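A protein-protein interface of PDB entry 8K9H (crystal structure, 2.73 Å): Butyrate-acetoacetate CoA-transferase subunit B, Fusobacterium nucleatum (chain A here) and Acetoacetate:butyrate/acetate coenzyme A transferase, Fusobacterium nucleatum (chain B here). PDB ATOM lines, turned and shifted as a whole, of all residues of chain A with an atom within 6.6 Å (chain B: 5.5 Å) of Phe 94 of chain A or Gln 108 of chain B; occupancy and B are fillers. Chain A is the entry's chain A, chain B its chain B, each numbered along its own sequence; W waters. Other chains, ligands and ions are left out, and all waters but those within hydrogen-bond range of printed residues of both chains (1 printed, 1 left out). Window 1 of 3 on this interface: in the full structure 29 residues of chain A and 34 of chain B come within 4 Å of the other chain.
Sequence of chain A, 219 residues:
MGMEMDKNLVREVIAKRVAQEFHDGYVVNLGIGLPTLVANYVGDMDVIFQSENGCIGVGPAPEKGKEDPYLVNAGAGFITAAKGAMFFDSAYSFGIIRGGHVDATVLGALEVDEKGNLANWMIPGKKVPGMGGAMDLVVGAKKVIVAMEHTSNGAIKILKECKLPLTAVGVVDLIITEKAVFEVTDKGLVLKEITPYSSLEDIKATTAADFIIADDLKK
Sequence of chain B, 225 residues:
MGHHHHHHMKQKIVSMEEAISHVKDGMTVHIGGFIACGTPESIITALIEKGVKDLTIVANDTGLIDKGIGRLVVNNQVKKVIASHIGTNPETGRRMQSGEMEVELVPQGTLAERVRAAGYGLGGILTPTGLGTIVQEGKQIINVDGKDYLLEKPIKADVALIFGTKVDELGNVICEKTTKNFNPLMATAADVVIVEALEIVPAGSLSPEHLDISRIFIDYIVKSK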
ATOM      1  N   GLN A  50       3.298   6.221  -8.830  1.00  0.00           N
ATOM      2  CA  GLN A  50       1.867   6.016  -8.754  1.00  0.00           C
ATOM      3  C   GLN A  50       1.533   5.472  -7.376  1.00  0.00           C
ATOM      4  O   GLN A  50       2.184   4.539  -6.902  1.00  0.00           O
ATOM      5  CB  GLN A  50       1.424   5.054  -9.864  1.00  0.00           C
ATOM      6  CG  GLN A  50      -0.057   5.089 -10.189  1.00  0.00           C
ATOM      7  CD  GLN A  50      -0.805   4.034  -9.422  1.00  0.00           C
ATOM      8  OE1 GLN A  50      -0.188   3.161  -8.817  1.00  0.00           O
ATOM      9  NE2 GLN A  50      -2.130   4.101  -9.434  1.00  0.00           N
ATOM     10  N   GLU A  52      -1.701   3.760  -5.380  1.00  0.00           N
ATOM     11  CA  GLU A  52      -2.973   3.050  -5.509  1.00  0.00           C
ATOM     12  C   GLU A  52      -4.190   3.911  -5.202  1.00  0.00           C
ATOM     13  O   GLU A  52      -5.228   3.756  -5.851  1.00  0.00           O
ATOM     14  CB  GLU A  52      -2.992   1.824  -4.576  1.00  0.00           C
ATOM     15  CG  GLU A  52      -1.615   1.193  -4.304  1.00  0.00           C
ATOM     16  CD  GLU A  52      -1.553   0.297  -3.043  1.00  0.00           C
ATOM     17  OE1 GLU A  52      -2.494   0.298  -2.206  1.00  0.00           O
ATOM     18  OE2 GLU A  52      -0.548  -0.440  -2.902  1.00  0.00           O
ATOM     19  N   ASN A  53      -4.100   4.801  -4.204  1.00  0.00           N
ATOM     20  CA  ASN A  53      -5.273   5.562  -3.770  1.00  0.00           C
ATOM     21  C   ASN A  53      -5.615   6.719  -4.701  1.00  0.00           C
ATOM     22  O   ASN A  53      -6.623   7.403  -4.483  1.00  0.00           O
ATOM     23  CB  ASN A  53      -5.095   6.069  -2.336  1.00  0.00           C
ATOM     24  CG  ASN A  53      -3.938   7.040  -2.193  1.00  0.00           C
ATOM     25  OD1 ASN A  53      -2.825   6.762  -2.639  1.00  0.00           O
ATOM     26  ND2 ASN A  53      -4.194   8.186  -1.556  1.00  0.00           N
ATOM     27  N   PHE A  88      -7.372  10.887  -9.574  1.00  0.00           N
ATOM     28  CA  PHE A  88      -8.421  10.035 -10.125  1.00  0.00           C
ATOM     29  C   PHE A  88      -8.955   9.065  -9.073  1.00  0.00           C
ATOM     30  O   PHE A  88      -8.347   8.855  -8.018  1.00  0.00           O
ATOM     31  CB  PHE A  88      -7.901   9.277 -11.337  1.00  0.00           C
ATOM     32  CG  PHE A  88      -6.512   8.747 -11.160  1.00  0.00           C
ATOM     33  CD1 PHE A  88      -6.266   7.643 -10.365  1.00  0.00           C
ATOM     34  CD2 PHE A  88      -5.444   9.349 -11.790  1.00  0.00           C
ATOM     35  CE1 PHE A  88      -4.971   7.148 -10.215  1.00  0.00           C
ATOM     36  CE2 PHE A  88      -4.165   8.854 -11.629  1.00  0.00           C
ATOM     37  CZ  PHE A  88      -3.934   7.754 -10.840  1.00  0.00           C
ATOM     38  N   ASP A  89     -10.109   8.459  -9.394  1.00  0.00           N
ATOM     39  CA  ASP A  89     -10.795   7.529  -8.508  1.00  0.00           C
ATOM     40  C   ASP A  89     -10.148   6.143  -8.554  1.00  0.00           C
ATOM     41  O   ASP A  89      -9.287   5.839  -9.389  1.00  0.00           O
ATOM     42  CB  ASP A  89     -12.300   7.446  -8.839  1.00  0.00           C
ATOM     43  CG  ASP A  89     -12.625   6.719 -10.189  1.00  0.00           C
ATOM     44  OD1 ASP A  89     -12.093   5.618 -10.498  1.00  0.00           O
ATOM     45  OD2 ASP A  89     -13.493   7.241 -10.933  1.00  0.00           O
ATOM     46  N   SER A  90     -10.616   5.282  -7.653  1.00  0.00           N
ATOM     47  CA  SER A  90      -9.962   4.003  -7.454  1.00  0.00           C
ATOM     48  C   SER A  90     -10.013   3.116  -8.700  1.00  0.00           C
ATOM     49  O   SER A  90      -9.065   2.350  -8.950  1.00  0.00           O
ATOM     50  CB  SER A  90     -10.572   3.307  -6.237  1.00  0.00           C
ATOM     51  OG  SER A  90      -9.793   3.611  -5.103  1.00  0.00           O
ATOM     52  N   ALA A  91     -11.086   3.204  -9.502  1.00  0.00           N
ATOM     53  CA  ALA A  91     -11.168   2.355 -10.689  1.00  0.00           C
ATOM     54  C   ALA A  91     -10.142   2.773 -11.747  1.00  0.00           C
ATOM     55  O   ALA A  91      -9.416   1.932 -12.298  1.00  0.00           O
ATOM     56  CB  ALA A  91     -12.585   2.370 -11.256  1.00  0.00           C
ATOM     57  N   TYR A  92     -10.050   4.076 -12.027  1.00  0.00           N
ATOM     58  CA  TYR A  92      -9.006   4.568 -12.921  1.00  0.00           C
ATOM     59  C   TYR A  92      -7.628   4.161 -12.420  1.00  0.00           C
ATOM     60  O   TYR A  92      -6.765   3.751 -13.207  1.00  0.00           O
ATOM     61  CB  TYR A  92      -9.112   6.085 -13.027  1.00  0.00           C
ATOM     62  CG  TYR A  92      -8.425   6.730 -14.194  1.00  0.00           C
ATOM     63  CD1 TYR A  92      -7.109   7.183 -14.096  1.00  0.00           C
ATOM     64  CD2 TYR A  92      -9.109   6.951 -15.383  1.00  0.00           C
ATOM     65  CE1 TYR A  92      -6.480   7.815 -15.170  1.00  0.00           C
ATOM     66  CE2 TYR A  92      -8.488   7.569 -16.469  1.00  0.00           C
ATOM     67  CZ  TYR A  92      -7.182   8.002 -16.357  1.00  0.00           C
ATOM     68  OH  TYR A  92      -6.595   8.615 -17.437  1.00  0.00           O
ATOM     69  N   SER A  93      -7.415   4.252 -11.105  1.00  0.00           N
ATOM     70  CA  SER A  93      -6.121   3.907 -10.528  1.00  0.00           C
ATOM     71  C   SER A  93      -5.756   2.467 -10.831  1.00  0.00           C
ATOM     72  O   SER A  93      -4.583   2.152 -11.079  1.00  0.00           O
ATOM     73  CB  SER A  93      -6.139   4.151  -9.014  1.00  0.00           C
ATOM     74  OG  SER A  93      -5.028   3.537  -8.394  1.00  0.00           O
ATOM     75  N   PHE A  94      -6.741   1.581 -10.814  1.00  0.00           N
ATOM     76  CA  PHE A  94      -6.411   0.192 -11.020  1.00  0.00           C
ATOM     77  C   PHE A  94      -6.557  -0.231 -12.473  1.00  0.00           C
ATOM     78  O   PHE A  94      -6.058  -1.302 -12.850  1.00  0.00           O
ATOM     79  CB  PHE A  94      -7.228  -0.665 -10.065  1.00  0.00           C
ATOM     80  CG  PHE A  94      -6.620  -0.741  -8.708  1.00  0.00           C
ATOM     81  CD1 PHE A  94      -5.597  -1.660  -8.446  1.00  0.00           C
ATOM     82  CD2 PHE A  94      -6.999   0.147  -7.716  1.00  0.00           C
ATOM     83  CE1 PHE A  94      -4.998  -1.729  -7.189  1.00  0.00           C
ATOM     84  CE2 PHE A  94      -6.408   0.099  -6.468  1.00  0.00           C
ATOM     85  CZ  PHE A  94      -5.400  -0.848  -6.199  1.00  0.00           C
ATOM     86  N   GLY A  95      -7.170   0.614 -13.303  1.00  0.00           N
ATOM     87  CA  GLY A  95      -6.952   0.501 -14.733  1.00  0.00           C
ATOM     88  C   GLY A  95      -5.496   0.719 -15.094  1.00  0.00           C
ATOM     89  O   GLY A  95      -4.916  -0.035 -15.874  1.00  0.00           O
ATOM     90  N   ILE A  96      -4.885   1.746 -14.510  1.00  0.00           N
ATOM     91  CA  ILE A  96      -3.457   1.971 -14.686  1.00  0.00           C
ATOM     92  C   ILE A  96      -2.664   0.769 -14.208  1.00  0.00           C
ATOM     93  O   ILE A  96      -1.706   0.340 -14.853  1.00  0.00           O
ATOM     94  CB  ILE A  96      -3.041   3.241 -13.932  1.00  0.00           C
ATOM     95  CG1 ILE A  96      -3.701   4.484 -14.565  1.00  0.00           C
ATOM     96  CG2 ILE A  96      -1.517   3.294 -13.815  1.00  0.00           C
ATOM     97  CD1 ILE A  96      -3.607   5.769 -13.706  1.00  0.00           C
ATOM     98  N   ILE A  97      -3.051   0.197 -13.074  1.00  0.00           N
ATOM     99  CA  ILE A  97      -2.265  -0.884 -12.484  1.00  0.00           C
ATOM    100  C   ILE A  97      -2.553  -2.207 -13.175  1.00  0.00           C
ATOM    101  O   ILE A  97      -1.632  -2.924 -13.578  1.00  0.00           O
ATOM    102  CB  ILE A  97      -2.545  -0.982 -10.974  1.00  0.00           C
ATOM    103  CG1 ILE A  97      -1.965   0.228 -10.249  1.00  0.00           C
ATOM    104  CG2 ILE A  97      -2.038  -2.305 -10.436  1.00  0.00           C
ATOM    105  CD1 ILE A  97      -2.724   0.600  -9.017  1.00  0.00           C
ATOM    106  N   ARG A  98      -3.833  -2.561 -13.307  1.00  0.00           N
ATOM    107  CA  ARG A  98      -4.169  -3.873 -13.838  1.00  0.00           C
ATOM    108  C   ARG A  98      -3.916  -3.948 -15.335  1.00  0.00           C
ATOM    109  O   ARG A  98      -3.673  -5.034 -15.865  1.00  0.00           O
ATOM    110  CB  ARG A  98      -5.628  -4.198 -13.525  1.00  0.00           C
ATOM    111  CG  ARG A  98      -6.065  -5.622 -13.795  1.00  0.00           C
ATOM    112  CD  ARG A  98      -7.522  -5.776 -13.436  1.00  0.00           C
ATOM    113  NE  ARG A  98      -8.209  -4.519 -13.698  1.00  0.00           N
ATOM    114  CZ  ARG A  98      -8.971  -3.854 -12.835  1.00  0.00           C
ATOM    115  NH1 ARG A  98      -9.195  -4.308 -11.608  1.00  0.00           N
ATOM    116  NH2 ARG A  98      -9.513  -2.712 -13.220  1.00  0.00           N
ATOM    117  N   GLY A  99      -3.968  -2.819 -16.036  1.00  0.00           N
ATOM    118  CA  GLY A  99      -3.819  -2.797 -17.472  1.00  0.00           C
ATOM    119  C   GLY A  99      -2.407  -2.692 -18.016  1.00  0.00           C
ATOM    120  O   GLY A  99      -2.238  -2.494 -19.221  1.00  0.00           O
ATOM    121  N   GLY A 100      -1.378  -2.808 -17.190  1.00  0.00           N
ATOM    122  CA  GLY A 100      -0.024  -2.867 -17.704  1.00  0.00           C
ATOM    123  C   GLY A 100       0.651  -1.536 -17.917  1.00  0.00           C
ATOM    124  O   GLY A 100       1.650  -1.472 -18.637  1.00  0.00           O
ATOM    125  N   MET A 131      -4.973  -7.877   1.202  1.00  0.00           N
ATOM    126  CA  MET A 131      -4.069  -7.819   0.071  1.00  0.00           C
ATOM    127  C   MET A 131      -3.885  -6.399  -0.451  1.00  0.00           C
ATOM    128  O   MET A 131      -2.966  -6.164  -1.253  1.00  0.00           O
ATOM    129  CB  MET A 131      -4.562  -8.753  -1.046  1.00  0.00           C
ATOM    130  CG  MET A 131      -5.979  -8.514  -1.554  1.00  0.00           C
ATOM    131  SD  MET A 131      -7.281  -9.024  -0.489  1.00  0.00           S
ATOM    132  CE  MET A 131      -6.851 -10.789  -0.517  1.00  0.00           C
ATOM    133  N   GLY A 132      -4.720  -5.462  -0.004  1.00  0.00           N
ATOM    134  CA  GLY A 132      -4.648  -4.105  -0.515  1.00  0.00           C
ATOM    135  C   GLY A 132      -4.667  -4.119  -2.025  1.00  0.00           C
ATOM    136  O   GLY A 132      -5.447  -4.853  -2.647  1.00  0.00           O
ATOM    137  N   GLY A 133      -3.782  -3.331  -2.630  1.00  0.00           N
ATOM    138  CA  GLY A 133      -3.607  -3.357  -4.065  1.00  0.00           C
ATOM    139  C   GLY A 133      -2.544  -4.311  -4.568  1.00  0.00           C
ATOM    140  O   GLY A 133      -2.267  -4.329  -5.768  1.00  0.00           O
ATOM    141  N   ALA A 134      -1.962  -5.139  -3.704  1.00  0.00           N
ATOM    142  CA  ALA A 134      -0.770  -5.889  -4.093  1.00  0.00           C
ATOM    143  C   ALA A 134      -1.070  -6.948  -5.159  1.00  0.00           C
ATOM    144  O   ALA A 134      -0.274  -7.130  -6.089  1.00  0.00           O
ATOM    145  CB  ALA A 134      -0.127  -6.542  -2.862  1.00  0.00           C
ATOM    146  N   MET A 135      -2.171  -7.703  -5.015  1.00  0.00           N
ATOM    147  CA  MET A 135      -2.523  -8.691  -6.035  1.00  0.00           C
ATOM    148  C   MET A 135      -2.638  -8.034  -7.399  1.00  0.00           C
ATOM    149  O   MET A 135      -2.113  -8.548  -8.397  1.00  0.00           O
ATOM    150  CB  MET A 135      -3.831  -9.446  -5.686  1.00  0.00           C
ATOM    151  CG  MET A 135      -3.630 -10.717  -4.903  1.00  0.00           C
ATOM    152  SD  MET A 135      -4.980 -11.541  -4.068  1.00  0.00           S
ATOM    153  CE  MET A 135      -5.952 -11.703  -5.451  1.00  0.00           C
ATOM    154  N   ASP A 136      -3.312  -6.888  -7.453  1.00  0.00           N
ATOM    155  CA  ASP A 136      -3.446  -6.183  -8.714  1.00  0.00           C
ATOM    156  C   ASP A 136      -2.097  -5.669  -9.206  1.00  0.00           C
ATOM    157  O   ASP A 136      -1.812  -5.706 -10.405  1.00  0.00           O
ATOM    158  CB  ASP A 136      -4.461  -5.062  -8.545  1.00  0.00           C
ATOM    159  CG  ASP A 136      -5.898  -5.595  -8.365  1.00  0.00           C
ATOM    160  OD1 ASP A 136      -6.451  -6.106  -9.367  1.00  0.00           O
ATOM    161  OD2 ASP A 136      -6.467  -5.517  -7.239  1.00  0.00           O
ATOM    162  N   LEU A 137      -1.226  -5.251  -8.296  1.00  0.00           N
ATOM    163  CA  LEU A 137       0.062  -4.703  -8.708  1.00  0.00           C
ATOM    164  C   LEU A 137       0.964  -5.777  -9.301  1.00  0.00           C
ATOM    165  O   LEU A 137       1.577  -5.570 -10.350  1.00  0.00           O
ATOM    166  CB  LEU A 137       0.751  -4.007  -7.529  1.00  0.00           C
ATOM    167  CG  LEU A 137       0.265  -2.596  -7.186  1.00  0.00           C
ATOM    168  CD1 LEU A 137       0.598  -2.270  -5.726  1.00  0.00           C
ATOM    169  CD2 LEU A 137       0.809  -1.558  -8.155  1.00  0.00           C
ATOM    170  N   PHE B  34     -10.319   6.284   1.770  1.00  0.00           N
ATOM    171  CA  PHE B  34      -9.083   5.504   1.744  1.00  0.00           C
ATOM    172  C   PHE B  34      -8.312   5.849   3.014  1.00  0.00           C
ATOM    173  O   PHE B  34      -7.768   6.948   3.138  1.00  0.00           O
ATOM    174  CB  PHE B  34      -8.259   5.794   0.487  1.00  0.00           C
ATOM    175  CG  PHE B  34      -7.072   4.888   0.318  1.00  0.00           C
ATOM    176  CD1 PHE B  34      -5.869   5.174   0.938  1.00  0.00           C
ATOM    177  CD2 PHE B  34      -7.157   3.747  -0.452  1.00  0.00           C
ATOM    178  CE1 PHE B  34      -4.776   4.343   0.787  1.00  0.00           C
ATOM    179  CE2 PHE B  34      -6.063   2.912  -0.603  1.00  0.00           C
ATOM    180  CZ  PHE B  34      -4.872   3.212   0.017  1.00  0.00           C
ATOM    181  N   ASN B  60     -12.978   0.490   1.017  1.00  0.00           N
ATOM    182  CA  ASN B  60     -11.583   0.139   0.757  1.00  0.00           C
ATOM    183  C   ASN B  60     -10.976  -0.542   1.970  1.00  0.00           C
ATOM    184  O   ASN B  60     -10.365  -1.612   1.861  1.00  0.00           O
ATOM    185  CB  ASN B  60     -10.768   1.379   0.393  1.00  0.00           C
ATOM    186  CG  ASN B  60      -9.303   1.054   0.135  1.00  0.00           C
ATOM    187  OD1 ASN B  60      -8.920   0.766  -0.994  1.00  0.00           O
ATOM    188  ND2 ASN B  60      -8.479   1.100   1.179  1.00  0.00           N
ATOM    189  N   SER B  84     -10.669  -4.351   1.187  1.00  0.00           N
ATOM    190  CA  SER B  84      -9.382  -4.819   0.681  1.00  0.00           C
ATOM    191  C   SER B  84      -8.307  -4.870   1.749  1.00  0.00           C
ATOM    192  O   SER B  84      -7.358  -5.655   1.636  1.00  0.00           O
ATOM    193  CB  SER B  84      -8.874  -3.925  -0.460  1.00  0.00           C
ATOM    194  OG  SER B  84      -8.815  -2.572  -0.080  1.00  0.00           O
ATOM    195  N   VAL B 106     -11.286  -8.397  -0.360  1.00  0.00           N
ATOM    196  CA  VAL B 106     -11.402  -8.243  -1.810  1.00  0.00           C
ATOM    197  C   VAL B 106     -10.192  -7.471  -2.322  1.00  0.00           C
ATOM    198  O   VAL B 106      -9.945  -6.361  -1.852  1.00  0.00           O
ATOM    199  CB  VAL B 106     -12.697  -7.501  -2.183  1.00  0.00           C
ATOM    200  CG1 VAL B 106     -12.821  -7.311  -3.698  1.00  0.00           C
ATOM    201  CG2 VAL B 106     -13.896  -8.208  -1.553  1.00  0.00           C
ATOM    202  N   PRO B 107      -9.463  -7.980  -3.319  1.00  0.00           N
ATOM    203  CA  PRO B 107      -8.408  -7.175  -3.957  1.00  0.00           C
ATOM    204  C   PRO B 107      -8.934  -5.825  -4.417  1.00  0.00           C
ATOM    205  O   PRO B 107     -10.003  -5.730  -5.024  1.00  0.00           O
ATOM    206  CB  PRO B 107      -7.980  -8.026  -5.156  1.00  0.00           C
ATOM    207  CG  PRO B 107      -8.397  -9.390  -4.836  1.00  0.00           C
ATOM    208  CD  PRO B 107      -9.651  -9.270  -4.002  1.00  0.00           C
ATOM    209  N   GLN B 108      -8.135  -4.787  -4.160  1.00  0.00           N
ATOM    210  CA  GLN B 108      -8.608  -3.412  -4.272  1.00  0.00           C
ATOM    211  C   GLN B 108      -9.106  -3.082  -5.674  1.00  0.00           C
ATOM    212  O   GLN B 108     -10.160  -2.455  -5.829  1.00  0.00           O
ATOM    213  CB  GLN B 108      -7.491  -2.477  -3.868  1.00  0.00           C
ATOM    214  CG  GLN B 108      -7.961  -1.148  -3.397  1.00  0.00           C
ATOM    215  CD  GLN B 108      -6.828  -0.333  -2.844  1.00  0.00           C
ATOM    216  OE1 GLN B 108      -6.539   0.761  -3.346  1.00  0.00           O
ATOM    217  NE2 GLN B 108      -6.176  -0.853  -1.798  1.00  0.00           N
ATOM    218  N   GLY B 109      -8.367  -3.483  -6.707  1.00  0.00           N
ATOM    219  CA  GLY B 109      -8.849  -3.258  -8.058  1.00  0.00           C
ATOM    220  C   GLY B 109     -10.123  -4.029  -8.366  1.00  0.00           C
ATOM    221  O   GLY B 109     -11.009  -3.541  -9.080  1.00  0.00           O
ATOM    222  N   THR B 110     -10.213  -5.258  -7.866  1.00  0.00           N
ATOM    223  CA  THR B 110     -11.443  -6.006  -7.999  1.00  0.00           C
ATOM    224  C   THR B 110     -12.565  -5.286  -7.280  1.00  0.00           C
ATOM    225  O   THR B 110     -13.689  -5.199  -7.792  1.00  0.00           O
ATOM    226  CB  THR B 110     -11.236  -7.413  -7.453  1.00  0.00           C
ATOM    227  OG1 THR B 110     -10.348  -8.116  -8.319  1.00  0.00           O
ATOM    228  CG2 THR B 110     -12.539  -8.165  -7.342  1.00  0.00           C
ATOM    229  N   LEU B 111     -12.274  -4.729  -6.103  1.00  0.00           N
ATOM    230  CA  LEU B 111     -13.317  -4.038  -5.351  1.00  0.00           C
ATOM    231  C   LEU B 111     -13.847  -2.854  -6.139  1.00  0.00           C
ATOM    232  O   LEU B 111     -15.056  -2.599  -6.155  1.00  0.00           O
ATOM    233  CB  LEU B 111     -12.795  -3.566  -3.991  1.00  0.00           C
ATOM    234  CG  LEU B 111     -13.888  -3.228  -2.973  1.00  0.00           C
ATOM    235  CD1 LEU B 111     -14.719  -4.463  -2.678  1.00  0.00           C
ATOM    236  CD2 LEU B 111     -13.286  -2.732  -1.713  1.00  0.00           C
ATOM    237  N   ALA B 112     -12.945  -2.115  -6.793  1.00  0.00           N
ATOM    238  CA  ALA B 112     -13.367  -0.989  -7.619  1.00  0.00           C
ATOM    239  C   ALA B 112     -14.293  -1.463  -8.729  1.00  0.00           C
ATOM    240  O   ALA B 112     -15.419  -0.964  -8.864  1.00  0.00           O
ATOM    241  CB  ALA B 112     -12.146  -0.259  -8.198  1.00  0.00           C
ATOM    242  N   GLU B 113     -13.843  -2.449  -9.519  1.00  0.00           N
ATOM    243  CA  GLU B 113     -14.674  -2.956 -10.602  1.00  0.00           C
ATOM    244  C   GLU B 113     -15.982  -3.573 -10.081  1.00  0.00           C
ATOM    245  O   GLU B 113     -17.025  -3.466 -10.740  1.00  0.00           O
ATOM    246  CB  GLU B 113     -13.870  -3.953 -11.431  1.00  0.00           C
ATOM    247  CG  GLU B 113     -12.711  -3.314 -12.214  1.00  0.00           C
ATOM    248  CD  GLU B 113     -13.142  -2.195 -13.181  1.00  0.00           C
ATOM    249  OE1 GLU B 113     -14.117  -2.374 -13.947  1.00  0.00           O
ATOM    250  OE2 GLU B 113     -12.501  -1.120 -13.176  1.00  0.00           O
ATOM    251  N   PHE B 182     -13.092   5.513  -3.865  1.00  0.00           N
ATOM    252  CA  PHE B 182     -14.294   4.857  -4.309  1.00  0.00           C
ATOM    253  C   PHE B 182     -15.512   5.763  -4.290  1.00  0.00           C
ATOM    254  O   PHE B 182     -16.569   5.346  -4.771  1.00  0.00           O
ATOM    255  CB  PHE B 182     -14.596   3.680  -3.405  1.00  0.00           C
ATOM    256  CG  PHE B 182     -13.643   2.550  -3.510  1.00  0.00           C
ATOM    257  CD1 PHE B 182     -12.368   2.656  -3.006  1.00  0.00           C
ATOM    258  CD2 PHE B 182     -14.052   1.345  -4.072  1.00  0.00           C
ATOM    259  CE1 PHE B 182     -11.487   1.593  -3.088  1.00  0.00           C
ATOM    260  CE2 PHE B 182     -13.185   0.277  -4.157  1.00  0.00           C
ATOM    261  CZ  PHE B 182     -11.892   0.397  -3.667  1.00  0.00           C
HETATM  262  O   HOH W   1      -8.650  -6.606 -10.541  1.00  0.00           O
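The backbone NH of Gly 132 of chain A is in hydrogen-bond range of the backbone carbonyl oxygen of Ser 84 of chain B (3.1 Å).
NH2 of Arg 98 of chain A is in salt-bridge range of OE2 of Glu 113 of chain B, 3.4 Å away.
SD of Met 131 of chain A lies close to N of Pro 107 of chain B.
NH1 of Arg 98 of chain A lies within hydrogen-bond range of O of Gly 109 of chain B.
N of Gly 109 of chain B is in hydrogen-bond range of OD2 of Asp 136 of chain A, 2.8 Å away.
The backbone NH (N) of Met 131 of chain A lies within hydrogen-bond range of the backbone carbonyl oxygen (O) of Ser 84 of chain B, at 3.3 Å.
N of Gln 108 of chain B lies within hydrogen-bond range of O of Gly 132 of chain A (3.1 Å).
The side-chain hydroxyl (OG) of Ser 84 of chain B lies within hydrogen-bond range of the backbone carbonyl oxygen (O) of Asn 60 of chain B (2.7 Å).
The side-chain carboxylate (OD1) of Asp 89 of chain A is in hydrogen-bond range of the backbone NH (N) of Ala 91 of chain A (2.8 Å).
OG of Ser 93 of chain A is in hydrogen-bond range of O of Glu 52 of chain A, at 2.6 Å.
The side-chain amide nitrogen (NE2) of Gln 108 of chain B sits close to the side-chain amide oxygen (OD1) of Asn 60 of chain B (3.3 Å).
OD1 of Asp 136 of chain A is in salt-bridge range of NH1 of Arg 98 of chain A (3.97 Å).
Among the printed residues, merely in contact across the chains: Phe 94 of chain A with Gln 108 of chain B (3.2 Å), Ser 90 of chain A with Phe 182 of chain B (3.3 Å), Met 135 of chain A with Pro 107 of chain B (3.4 Å), Phe 94 of chain A with Gly 109 of chain B (3.4 Å), Asn 53 of chain A with Phe 34 of chain B (3.5 Å), Gly 133 of chain A with Gln 108 of chain B (3.5 Å), Asp 136 of chain A with Gln 108 of chain B (3.6 Å), Asp 136 of chain A with Pro 107 of chain B (3.6 Å), Ala 91 of chain A with Ala 112 of chain B (3.7 Å), Met 131 of chain A with Val 106 of chain B (3.8 Å), Asp 136 of chain A with Thr 110 of chain B (3.8 Å), Glu 52 of chain A with Gln 108 of chain B (3.9 Å), Ala 91 of chain A with Glu 113 of chain B (3.98 Å), Gly 132 of chain A with Pro 107 of chain B (3.98 Å) and Arg 98 of chain A with Thr 110 of chain B (3.99 Å).
Printed residues of chain B within 4 Å of Ser 90 of chain A: Phe 182.
Phe 94 of chain A touches two residues of chain B.
Ile 96 of chain A touches none of the printed residues of chain B.
Ile 97 of chain A touches none of the printed residues of chain B.
Printed residues of chain A within 4 Å of Phe 34 of chain B: Asn 53.
Of the printed residues of chain A, Val 106 of chain B touches Met 131 (3.8 Å).
Gln 108 of chain B touches just these residues of chain A: Glu 52, Phe 94, Gly 132, Gly 133 and Asp 136.
Printed residues of chain A within 4 Å of Ala 112 of chain B: Ala 91 (3.7 Å).
Of the printed residues of chain A, Phe 182 of chain B touches Ser 90 (3.3 Å).
The nearest residue of chain B that does not touch Phe 94 of chain A is Ala 112 of chain B (5.2 Å).
The nearest residue of chain A that does not touch Gln 108 of chain B is Ser 90 of chain A (4.7 Å).
Hydrophobic or aromatic side chains of chain A within 4 Å of the printed part of chain B: Ala 91, Phe 94, Met 131 and Met 135.
Of the 12 printed residues of chain B, 10 touch a printed residue of chain A.
Along chain B the printed residues that touch a printed residue of chain A span positions 34 to 182.
Among the printed residues, 22 pairs touch across the chains.
Among the printed residues, Asp or Glu carboxylates within 4 Å of a Lys or Arg side-chain nitrogen of the other chain: Arg 98 of chain A with Glu 113 of chain B (3.4 Å).
Water W1 lies within hydrogen-bond range of the side-chain carboxylate (OD1) of Asp 136 of chain A (2.5 Å), the guanidinium group (NH1) of Arg 98 of chain A (2.6 Å) and the side-chain hydroxyl (OG1) of Thr 110 of chain B (3.2 Å).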
